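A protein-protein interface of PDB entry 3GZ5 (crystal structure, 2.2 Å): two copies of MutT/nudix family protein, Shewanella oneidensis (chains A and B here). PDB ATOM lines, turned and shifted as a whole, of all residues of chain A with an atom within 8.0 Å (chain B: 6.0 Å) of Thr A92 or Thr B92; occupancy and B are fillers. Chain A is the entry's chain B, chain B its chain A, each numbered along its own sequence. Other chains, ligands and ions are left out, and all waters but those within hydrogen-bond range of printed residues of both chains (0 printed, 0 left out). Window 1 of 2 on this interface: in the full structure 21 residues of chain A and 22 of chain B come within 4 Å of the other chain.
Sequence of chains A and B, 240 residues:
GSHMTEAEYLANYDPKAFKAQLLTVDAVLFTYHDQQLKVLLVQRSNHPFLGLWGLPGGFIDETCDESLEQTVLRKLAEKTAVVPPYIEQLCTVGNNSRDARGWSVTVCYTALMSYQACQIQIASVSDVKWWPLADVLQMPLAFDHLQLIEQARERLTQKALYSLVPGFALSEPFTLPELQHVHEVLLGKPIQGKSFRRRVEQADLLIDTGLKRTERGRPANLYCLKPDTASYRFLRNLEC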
ATOM      1  N   LEU A  23      20.410   8.265  22.252  1.00  0.00           N
ATOM      2  CA  LEU A  23      21.197   7.767  21.151  1.00  0.00           C
ATOM      3  C   LEU A  23      21.658   8.961  20.357  1.00  0.00           C
ATOM      4  O   LEU A  23      20.837   9.698  19.829  1.00  0.00           O
ATOM      5  CB  LEU A  23      20.349   6.831  20.286  1.00  0.00           C
ATOM      6  CG  LEU A  23      20.964   6.185  19.042  1.00  0.00           C
ATOM      7  CD1 LEU A  23      22.185   5.329  19.399  1.00  0.00           C
ATOM      8  CD2 LEU A  23      19.896   5.340  18.291  1.00  0.00           C
ATOM      9  N   THR A  24      22.972   9.170  20.314  1.00  0.00           N
ATOM     10  CA  THR A  24      23.545  10.282  19.573  1.00  0.00           C
ATOM     11  C   THR A  24      24.659   9.819  18.630  1.00  0.00           C
ATOM     12  O   THR A  24      25.118   8.668  18.681  1.00  0.00           O
ATOM     13  CB  THR A  24      24.074  11.392  20.505  1.00  0.00           C
ATOM     14  OG1 THR A  24      25.111  10.864  21.345  1.00  0.00           O
ATOM     15  CG2 THR A  24      22.928  12.002  21.389  1.00  0.00           C
ATOM     16  N   VAL A  25      25.075  10.711  17.748  1.00  0.00           N
ATOM     17  CA  VAL A  25      26.219  10.455  16.900  1.00  0.00           C
ATOM     18  C   VAL A  25      27.179  11.618  17.203  1.00  0.00           C
ATOM     19  O   VAL A  25      26.708  12.719  17.412  1.00  0.00           O
ATOM     20  CB  VAL A  25      25.778  10.359  15.381  1.00  0.00           C
ATOM     21  CG1 VAL A  25      26.931  10.006  14.498  1.00  0.00           C
ATOM     22  CG2 VAL A  25      24.706   9.289  15.199  1.00  0.00           C
ATOM     23  N   LEU A  68      23.531   6.504   9.448  1.00  0.00           N
ATOM     24  CA  LEU A  68      24.369   7.125  10.481  1.00  0.00           C
ATOM     25  C   LEU A  68      25.430   8.063   9.917  1.00  0.00           C
ATOM     26  O   LEU A  68      25.675   9.111  10.490  1.00  0.00           O
ATOM     27  CB  LEU A  68      25.013   6.058  11.341  1.00  0.00           C
ATOM     28  CG  LEU A  68      24.046   5.251  12.214  1.00  0.00           C
ATOM     29  CD1 LEU A  68      24.837   4.144  12.843  1.00  0.00           C
ATOM     30  CD2 LEU A  68      23.332   6.164  13.260  1.00  0.00           C
ATOM     31  N   GLU A  69      26.035   7.713   8.786  1.00  0.00           N
ATOM     32  CA  GLU A  69      26.962   8.623   8.119  1.00  0.00           C
ATOM     33  C   GLU A  69      26.300   9.944   7.713  1.00  0.00           C
ATOM     34  O   GLU A  69      26.892  11.022   7.883  1.00  0.00           O
ATOM     35  CB  GLU A  69      27.655   7.963   6.911  1.00  0.00           C
ATOM     36  CG  GLU A  69      28.796   8.795   6.349  1.00  0.00           C
ATOM     37  CD  GLU A  69      29.391   8.211   5.074  1.00  0.00           C
ATOM     38  OE1 GLU A  69      29.108   8.746   3.982  1.00  0.00           O
ATOM     39  OE2 GLU A  69      30.137   7.212   5.159  1.00  0.00           O
ATOM     40  N   GLN A  89      33.927   5.709  11.042  1.00  0.00           N
ATOM     41  CA  GLN A  89      33.443   5.369  12.369  1.00  0.00           C
ATOM     42  C   GLN A  89      34.601   4.947  13.284  1.00  0.00           C
ATOM     43  O   GLN A  89      35.445   4.121  12.906  1.00  0.00           O
ATOM     44  CB  GLN A  89      32.402   4.248  12.249  1.00  0.00           C
ATOM     45  CG  GLN A  89      31.273   4.305  13.252  1.00  0.00           C
ATOM     46  CD  GLN A  89      30.244   3.220  13.019  1.00  0.00           C
ATOM     47  OE1 GLN A  89      29.195   3.452  12.397  1.00  0.00           O
ATOM     48  NE2 GLN A  89      30.529   2.045  13.517  1.00  0.00           N
ATOM     49  N   LEU A  90      34.658   5.533  14.476  1.00  0.00           N
ATOM     50  CA  LEU A  90      35.650   5.202  15.486  1.00  0.00           C
ATOM     51  C   LEU A  90      35.192   4.052  16.411  1.00  0.00           C
ATOM     52  O   LEU A  90      35.817   2.991  16.494  1.00  0.00           O
ATOM     53  CB  LEU A  90      35.971   6.459  16.311  1.00  0.00           C
ATOM     54  CG  LEU A  90      37.042   6.333  17.408  1.00  0.00           C
ATOM     55  CD1 LEU A  90      38.404   5.944  16.835  1.00  0.00           C
ATOM     56  CD2 LEU A  90      37.140   7.589  18.304  1.00  0.00           C
ATOM     57  N   CYS A  91      34.089   4.285  17.118  1.00  0.00           N
ATOM     58  CA  CYS A  91      33.629   3.383  18.137  1.00  0.00           C
ATOM     59  C   CYS A  91      32.211   3.818  18.533  1.00  0.00           C
ATOM     60  O   CYS A  91      31.751   4.911  18.162  1.00  0.00           O
ATOM     61  CB  CYS A  91      34.574   3.393  19.354  1.00  0.00           C
ATOM     62  SG  CYS A  91      34.669   5.016  20.150  1.00  0.00           S
ATOM     63  N   THR A  92      31.511   2.926  19.225  1.00  0.00           N
ATOM     64  CA  THR A  92      30.192   3.207  19.780  1.00  0.00           C
ATOM     65  C   THR A  92      30.368   2.982  21.260  1.00  0.00           C
ATOM     66  O   THR A  92      30.794   1.913  21.676  1.00  0.00           O
ATOM     67  CB  THR A  92      29.117   2.273  19.166  1.00  0.00           C
ATOM     68  OG1 THR A  92      28.968   2.623  17.788  1.00  0.00           O
ATOM     69  CG2 THR A  92      27.763   2.422  19.848  1.00  0.00           C
ATOM     70  N   VAL A  93      30.115   4.015  22.051  1.00  0.00           N
ATOM     71  CA  VAL A  93      30.158   3.853  23.506  1.00  0.00           C
ATOM     72  C   VAL A  93      28.737   3.878  24.068  1.00  0.00           C
ATOM     73  O   VAL A  93      27.921   4.739  23.697  1.00  0.00           O
ATOM     74  CB  VAL A  93      31.051   4.917  24.176  1.00  0.00           C
ATOM     75  CG1 VAL A  93      31.061   4.725  25.683  1.00  0.00           C
ATOM     76  CG2 VAL A  93      32.497   4.763  23.676  1.00  0.00           C
ATOM     77  N   GLY A  94      28.445   2.943  24.967  1.00  0.00           N
ATOM     78  CA  GLY A  94      27.122   2.905  25.583  1.00  0.00           C
ATOM     79  C   GLY A  94      27.150   2.219  26.924  1.00  0.00           C
ATOM     80  O   GLY A  94      27.610   1.095  27.027  1.00  0.00           O
ATOM     81  N   ASN A  95      26.669   2.919  27.945  1.00  0.00           N
ATOM     82  CA  ASN A  95      26.600   2.426  29.308  1.00  0.00           C
ATOM     83  C   ASN A  95      25.704   3.341  30.161  1.00  0.00           C
ATOM     84  O   ASN A  95      25.164   4.355  29.664  1.00  0.00           O
ATOM     85  CB  ASN A  95      28.015   2.314  29.910  1.00  0.00           C
ATOM     86  CG  ASN A  95      28.752   3.650  29.935  1.00  0.00           C
ATOM     87  OD1 ASN A  95      29.856   3.783  29.411  1.00  0.00           O
ATOM     88  ND2 ASN A  95      28.128   4.645  30.522  1.00  0.00           N
ATOM     89  N   ARG A  98      27.935   7.103  31.824  1.00  0.00           N
ATOM     90  CA  ARG A  98      28.568   8.212  31.095  1.00  0.00           C
ATOM     91  C   ARG A  98      27.672   9.446  31.030  1.00  0.00           C
ATOM     92  O   ARG A  98      28.137  10.550  30.755  1.00  0.00           O
ATOM     93  CB  ARG A  98      28.998   7.786  29.669  1.00  0.00           C
ATOM     94  CG  ARG A  98      27.857   7.362  28.731  1.00  0.00           C
ATOM     95  CD  ARG A  98      28.377   6.803  27.379  1.00  0.00           C
ATOM     96  NE  ARG A  98      29.052   7.809  26.557  1.00  0.00           N
ATOM     97  CZ  ARG A  98      28.424   8.718  25.820  1.00  0.00           C
ATOM     98  NH1 ARG A  98      27.097   8.764  25.806  1.00  0.00           N
ATOM     99  NH2 ARG A  98      29.116   9.598  25.114  1.00  0.00           N
ATOM    100  N   SER A 104      22.901   5.849  27.942  1.00  0.00           N
ATOM    101  CA  SER A 104      23.071   6.519  26.643  1.00  0.00           C
ATOM    102  C   SER A 104      24.113   5.830  25.770  1.00  0.00           C
ATOM    103  O   SER A 104      25.080   5.242  26.276  1.00  0.00           O
ATOM    104  CB  SER A 104      23.454   7.973  26.818  1.00  0.00           C
ATOM    105  OG  SER A 104      24.790   8.043  27.229  1.00  0.00           O
ATOM    106  N   VAL A 105      23.891   5.921  24.464  1.00  0.00           N
ATOM    107  CA  VAL A 105      24.750   5.319  23.466  1.00  0.00           C
ATOM    108  C   VAL A 105      25.199   6.394  22.495  1.00  0.00           C
ATOM    109  O   VAL A 105      24.384   7.154  22.002  1.00  0.00           O
ATOM    110  CB  VAL A 105      24.008   4.167  22.716  1.00  0.00           C
ATOM    111  CG1 VAL A 105      24.860   3.604  21.598  1.00  0.00           C
ATOM    112  CG2 VAL A 105      23.642   3.058  23.691  1.00  0.00           C
ATOM    113  N   THR A 106      26.490   6.460  22.226  1.00  0.00           N
ATOM    114  CA  THR A 106      26.998   7.403  21.256  1.00  0.00           C
ATOM    115  C   THR A 106      27.841   6.694  20.175  1.00  0.00           C
ATOM    116  O   THR A 106      28.793   5.966  20.475  1.00  0.00           O
ATOM    117  CB  THR A 106      27.792   8.595  21.927  1.00  0.00           C
ATOM    118  OG1 THR A 106      27.658   9.778  21.117  1.00  0.00           O
ATOM    119  CG2 THR A 106      29.240   8.284  22.013  1.00  0.00           C
ATOM    120  N   VAL A 107      27.467   6.907  18.920  1.00  0.00           N
ATOM    121  CA  VAL A 107      28.242   6.400  17.802  1.00  0.00           C
ATOM    122  C   VAL A 107      29.254   7.487  17.396  1.00  0.00           C
ATOM    123  O   VAL A 107      28.877   8.582  16.940  1.00  0.00           O
ATOM    124  CB  VAL A 107      27.333   5.977  16.636  1.00  0.00           C
ATOM    125  CG1 VAL A 107      28.159   5.310  15.537  1.00  0.00           C
ATOM    126  CG2 VAL A 107      26.180   5.054  17.148  1.00  0.00           C
ATOM    127  N   CYS A 108      30.530   7.194  17.623  1.00  0.00           N
ATOM    128  CA  CYS A 108      31.606   8.161  17.425  1.00  0.00           C
ATOM    129  C   CYS A 108      32.354   7.918  16.145  1.00  0.00           C
ATOM    130  O   CYS A 108      32.685   6.779  15.830  1.00  0.00           O
ATOM    131  CB  CYS A 108      32.601   8.178  18.605  1.00  0.00           C
ATOM    132  SG  CYS A 108      33.642   9.719  18.568  1.00  0.00           S
ATOM    133  N   TYR A 109      32.596   9.009  15.413  1.00  0.00           N
ATOM    134  CA  TYR A 109      33.312   9.039  14.144  1.00  0.00           C
ATOM    135  C   TYR A 109      34.598   9.844  14.303  1.00  0.00           C
ATOM    136  O   TYR A 109      34.671  10.723  15.192  1.00  0.00           O
ATOM    137  CB  TYR A 109      32.454   9.718  13.062  1.00  0.00           C
ATOM    138  CG  TYR A 109      31.320   8.840  12.559  1.00  0.00           C
ATOM    139  CD1 TYR A 109      31.434   8.161  11.347  1.00  0.00           C
ATOM    140  CD2 TYR A 109      30.170   8.660  13.307  1.00  0.00           C
ATOM    141  CE1 TYR A 109      30.418   7.332  10.882  1.00  0.00           C
ATOM    142  CE2 TYR A 109      29.142   7.815  12.861  1.00  0.00           C
ATOM    143  CZ  TYR A 109      29.274   7.167  11.649  1.00  0.00           C
ATOM    144  OH  TYR A 109      28.277   6.334  11.197  1.00  0.00           O
ATOM    145  N   ASP A 144      32.133  12.192  28.265  1.00  0.00           N
ATOM    146  CA  ASP A 144      33.342  11.382  28.179  1.00  0.00           C
ATOM    147  C   ASP A 144      34.109  11.749  26.911  1.00  0.00           C
ATOM    148  O   ASP A 144      34.929  10.960  26.432  1.00  0.00           O
ATOM    149  CB  ASP A 144      32.995   9.871  28.203  1.00  0.00           C
ATOM    150  CG  ASP A 144      32.072   9.441  27.032  1.00  0.00           C
ATOM    151  OD1 ASP A 144      31.521  10.307  26.315  1.00  0.00           O
ATOM    152  OD2 ASP A 144      31.890   8.226  26.846  1.00  0.00           O
ATOM    153  N   LEU A 148      36.940  10.004  24.125  1.00  0.00           N
ATOM    154  CA  LEU A 148      36.686   9.818  22.686  1.00  0.00           C
ATOM    155  C   LEU A 148      37.761  10.494  21.807  1.00  0.00           C
ATOM    156  O   LEU A 148      38.207   9.920  20.822  1.00  0.00           O
ATOM    157  CB  LEU A 148      35.280  10.318  22.313  1.00  0.00           C
ATOM    158  CG  LEU A 148      34.053   9.546  22.830  1.00  0.00           C
ATOM    159  CD1 LEU A 148      32.786  10.273  22.473  1.00  0.00           C
ATOM    160  CD2 LEU A 148      33.986   8.076  22.325  1.00  0.00           C
ATOM    161  N   GLN A 151      40.960   8.382  22.053  1.00  0.00           N
ATOM    162  CA  GLN A 151      40.794   7.227  21.194  1.00  0.00           C
ATOM    163  C   GLN A 151      40.957   7.596  19.694  1.00  0.00           C
ATOM    164  O   GLN A 151      41.660   6.909  18.954  1.00  0.00           O
ATOM    165  CB  GLN A 151      39.452   6.555  21.476  1.00  0.00           C
ATOM    166  CG  GLN A 151      39.414   5.091  21.062  1.00  0.00           C
ATOM    167  CD  GLN A 151      38.222   4.328  21.629  1.00  0.00           C
ATOM    168  OE1 GLN A 151      37.631   4.708  22.657  1.00  0.00           O
ATOM    169  NE2 GLN A 151      37.866   3.233  20.956  1.00  0.00           N
ATOM    170  N   LEU B  68      27.290  -1.785  26.715  1.00  0.00           N
ATOM    171  CA  LEU B  68      27.037  -2.519  25.464  1.00  0.00           C
ATOM    172  C   LEU B  68      27.691  -3.898  25.451  1.00  0.00           C
ATOM    173  O   LEU B  68      27.076  -4.864  25.014  1.00  0.00           O
ATOM    174  CB  LEU B  68      27.465  -1.694  24.249  1.00  0.00           C
ATOM    175  CG  LEU B  68      26.582  -0.478  23.980  1.00  0.00           C
ATOM    176  CD1 LEU B  68      27.200   0.355  22.856  1.00  0.00           C
ATOM    177  CD2 LEU B  68      25.180  -0.904  23.613  1.00  0.00           C
ATOM    178  N   GLN B  89      34.201  -5.117  19.486  1.00  0.00           N
ATOM    179  CA  GLN B  89      33.216  -4.363  18.731  1.00  0.00           C
ATOM    180  C   GLN B  89      33.637  -4.226  17.287  1.00  0.00           C
ATOM    181  O   GLN B  89      34.808  -3.933  17.011  1.00  0.00           O
ATOM    182  CB  GLN B  89      33.003  -2.979  19.329  1.00  0.00           C
ATOM    183  CG  GLN B  89      31.704  -2.319  18.920  1.00  0.00           C
ATOM    184  CD  GLN B  89      31.521  -0.981  19.597  1.00  0.00           C
ATOM    185  OE1 GLN B  89      30.815  -0.871  20.615  1.00  0.00           O
ATOM    186  NE2 GLN B  89      32.172   0.038  19.069  1.00  0.00           N
ATOM    187  N   LEU B  90      32.663  -4.390  16.378  1.00  0.00           N
ATOM    188  CA  LEU B  90      32.937  -4.394  14.940  1.00  0.00           C
ATOM    189  C   LEU B  90      32.574  -3.080  14.215  1.00  0.00           C
ATOM    190  O   LEU B  90      33.418  -2.467  13.545  1.00  0.00           O
ATOM    191  CB  LEU B  90      32.263  -5.602  14.263  1.00  0.00           C
ATOM    192  CG  LEU B  90      32.389  -5.687  12.728  1.00  0.00           C
ATOM    193  CD1 LEU B  90      33.856  -5.846  12.268  1.00  0.00           C
ATOM    194  CD2 LEU B  90      31.513  -6.790  12.133  1.00  0.00           C
ATOM    195  N   CYS B  91      31.314  -2.667  14.330  1.00  0.00           N
ATOM    196  CA  CYS B  91      30.804  -1.489  13.628  1.00  0.00           C
ATOM    197  C   CYS B  91      29.387  -1.306  14.115  1.00  0.00           C
ATOM    198  O   CYS B  91      28.805  -2.231  14.701  1.00  0.00           O
ATOM    199  CB  CYS B  91      30.783  -1.715  12.102  1.00  0.00           C
ATOM    200  SG  CYS B  91      29.697  -3.084  11.605  1.00  0.00           S
ATOM    201  N   THR B  92      28.832  -0.120  13.886  1.00  0.00           N
ATOM    202  CA  THR B  92      27.436   0.136  14.177  1.00  0.00           C
ATOM    203  C   THR B  92      26.812   0.491  12.849  1.00  0.00           C
ATOM    204  O   THR B  92      27.308   1.356  12.121  1.00  0.00           O
ATOM    205  CB  THR B  92      27.254   1.274  15.242  1.00  0.00           C
ATOM    206  OG1 THR B  92      27.899   0.880  16.451  1.00  0.00           O
ATOM    207  CG2 THR B  92      25.786   1.555  15.537  1.00  0.00           C
ATOM    208  N   VAL B  93      25.734  -0.225  12.533  1.00  0.00           N
ATOM    209  CA  VAL B  93      24.965   0.005  11.317  1.00  0.00           C
ATOM    210  C   VAL B  93      23.652   0.631  11.746  1.00  0.00           C
ATOM    211  O   VAL B  93      23.024   0.178  12.706  1.00  0.00           O
ATOM    212  CB  VAL B  93      24.678  -1.327  10.573  1.00  0.00           C
ATOM    213  CG1 VAL B  93      23.950  -1.074   9.271  1.00  0.00           C
ATOM    214  CG2 VAL B  93      25.985  -2.033  10.293  1.00  0.00           C
ATOM    215  N   GLY B  94      23.235   1.665  11.037  1.00  0.00           N
ATOM    216  CA  GLY B  94      21.975   2.333  11.324  1.00  0.00           C
ATOM    217  C   GLY B  94      21.516   3.012  10.058  1.00  0.00           C
ATOM    218  O   GLY B  94      22.291   3.759   9.419  1.00  0.00           O
ATOM    219  N   VAL B 105      19.042   0.734  14.340  1.00  0.00           N
ATOM    220  CA  VAL B 105      20.460   0.803  14.649  1.00  0.00           C
ATOM    221  C   VAL B 105      20.904  -0.489  15.354  1.00  0.00           C
ATOM    222  O   VAL B 105      20.260  -0.927  16.303  1.00  0.00           O
ATOM    223  CB  VAL B 105      20.817   2.047  15.534  1.00  0.00           C
ATOM    224  CG1 VAL B 105      22.315   2.065  15.903  1.00  0.00           C
ATOM    225  CG2 VAL B 105      20.435   3.352  14.853  1.00  0.00           C
ATOM    226  N   THR B 106      21.994  -1.099  14.873  1.00  0.00           N
ATOM    227  CA  THR B 106      22.573  -2.263  15.524  1.00  0.00           C
ATOM    228  C   THR B 106      24.084  -2.112  15.720  1.00  0.00           C
ATOM    229  O   THR B 106      24.817  -1.840  14.777  1.00  0.00           O
ATOM    230  CB  THR B 106      22.240  -3.643  14.793  1.00  0.00           C
ATOM    231  OG1 THR B 106      22.475  -4.720  15.707  1.00  0.00           O
ATOM    232  CG2 THR B 106      23.170  -3.903  13.636  1.00  0.00           C
ATOM    233  N   VAL B 107      24.521  -2.267  16.972  1.00  0.00           N
ATOM    234  CA  VAL B 107      25.928  -2.299  17.310  1.00  0.00           C
ATOM    235  C   VAL B 107      26.418  -3.752  17.206  1.00  0.00           C
ATOM    236  O   VAL B 107      25.993  -4.632  17.978  1.00  0.00           O
ATOM    237  CB  VAL B 107      26.206  -1.787  18.738  1.00  0.00           C
ATOM    238  CG1 VAL B 107      27.720  -1.637  18.949  1.00  0.00           C
ATOM    239  CG2 VAL B 107      25.449  -0.492  19.019  1.00  0.00           C
ATOM    240  N   CYS B 108      27.315  -3.995  16.263  1.00  0.00           N
ATOM    241  CA  CYS B 108      27.779  -5.361  16.000  1.00  0.00           C
ATOM    242  C   CYS B 108      29.128  -5.655  16.647  1.00  0.00           C
ATOM    243  O   CYS B 108      30.017  -4.809  16.644  1.00  0.00           O
ATOM    244  CB  CYS B 108      27.802  -5.658  14.483  1.00  0.00           C
ATOM    245  SG  CYS B 108      27.912  -7.437  14.084  1.00  0.00           S
ATOM    246  N   TYR B 109      29.278  -6.879  17.156  1.00  0.00           N
ATOM    247  CA  TYR B 109      30.534  -7.388  17.710  1.00  0.00           C
ATOM    248  C   TYR B 109      31.023  -8.614  16.937  1.00  0.00           C
ATOM    249  O   TYR B 109      30.216  -9.326  16.321  1.00  0.00           O
ATOM    250  CB  TYR B 109      30.344  -7.764  19.199  1.00  0.00           C
ATOM    251  CG  TYR B 109      30.116  -6.535  20.098  1.00  0.00           C
ATOM    252  CD1 TYR B 109      31.118  -6.105  20.979  1.00  0.00           C
ATOM    253  CD2 TYR B 109      28.938  -5.773  20.018  1.00  0.00           C
ATOM    254  CE1 TYR B 109      30.950  -5.011  21.763  1.00  0.00           C
ATOM    255  CE2 TYR B 109      28.764  -4.656  20.809  1.00  0.00           C
ATOM    256  CZ  TYR B 109      29.796  -4.281  21.674  1.00  0.00           C
ATOM    257  OH  TYR B 109      29.690  -3.184  22.478  1.00  0.00           O
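Printed residues of chain A that touch a printed residue of chain B: Leu A68, Gln A89, Cys A91, Thr A92, Gly A94 and Val A107.
Hydrophobic or aromatic side chains of chain A that line the printed part of chain B: Leu A68 and Val A107.
Hydrophobic or aromatic side chains of chain B within 4 Å of the printed part of chain A: Leu B68 and Val B107.
Among the printed residues, 12 pairs touch across the chains.
Among the printed residues, no Asp or Glu carboxylate lies within 4 Å of a Lys or Arg side-chain nitrogen of the other chain.
The backbone NH (N) of Thr B106 sits at hydrogen-bond distance from the backbone carbonyl oxygen (O) of Val B93 (2.7 Å).
O of Cys A91 is in hydrogen-bond range of N of Cys A108, 2.6 Å away.
The side-chain amide oxygen (OE1) of Gln A89 lies within hydrogen-bond range of the side-chain hydroxyl (OH) of Tyr A109 (3.3 Å).
The backbone carbonyl oxygen of Cys B91 is in hydrogen-bond range of the backbone NH of Cys B108, at 2.8 Å.
OE1 of Gln B89 lies within hydrogen-bond range of OH of Tyr B109, 3.2 Å away.
The side-chain sulfur (SG) of Cys A91 sits close to the side-chain amide nitrogen (NE2) of Gln A151.
Leu A68 touches Gly B94, and with the chains exchanged Gly A94 touches Leu B68.
Gln A89 touches Cys B91, and with the chains exchanged Cys A91 touches Gln B89.
Gln A89 touches Thr B92, and with the chains exchanged Thr A92 touches Gln B89.
Thr A92 touches Val B107, and with the chains exchanged Val A107 touches Thr B92.
Among the printed residues, merely in contact across the chains: Gln A89 with Cys B91 (3.5 Å), Thr A92 with Leu B68 (3.7 Å), Cys A91 with Gln B89 (3.8 Å), Leu A68 with Thr B92 (3.8 Å), Thr A92 with Val B107 (3.8 Å), Leu A68 with Val B93 (3.9 Å) and Val A107 with Thr B92 (3.9 Å).
Thr A92 touches four residues of chain B.
Of chain A, only Leu A68 (3.8 Å), Gln A89 (2.8 Å), Thr A92 (2.4 Å) and Val A107 (3.9 Å) come within 4 Å of Thr B92.
Of the printed residues of chain B, Leu A68 touches Thr B92 (3.8 Å), Val B93 (3.9 Å) and Gly B94 (3.0 Å).
Printed residues of chain B within 4 Å of Gln A89: Cys B91 and Thr B92.
Printed residues of chain A within 4 Å of Gly B94: Leu A68.
Printed residues of chain A within 4 Å of Val B93: Leu A68 (3.9 Å).
Of the printed residues of chain B, Val A107 touches Thr B92.
The nearest residue of chain B that does not touch Thr A92 is Tyr B109 (5.3 Å).
The nearest residue of chain A that does not touch Thr B92 is Tyr A109 (5.2 Å).
NE2 of Gln B89 lies close to N of Thr A92, 3.0 Å away.
The side-chain amide nitrogen (NE2) of Gln A89 sits close to the backbone NH (N) of Thr B92 (2.8 Å).
The side-chain hydroxyl of Thr A92 sits at hydrogen-bond distance from the side-chain hydroxyl of Thr B92 (2.4 Å).
N of Leu A68 is in hydrogen-bond range of O of Gly B94 (3.0 Å).
The backbone NH (N) of Leu B68 is in hydrogen-bond range of the backbone carbonyl oxygen (O) of Gly A94.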
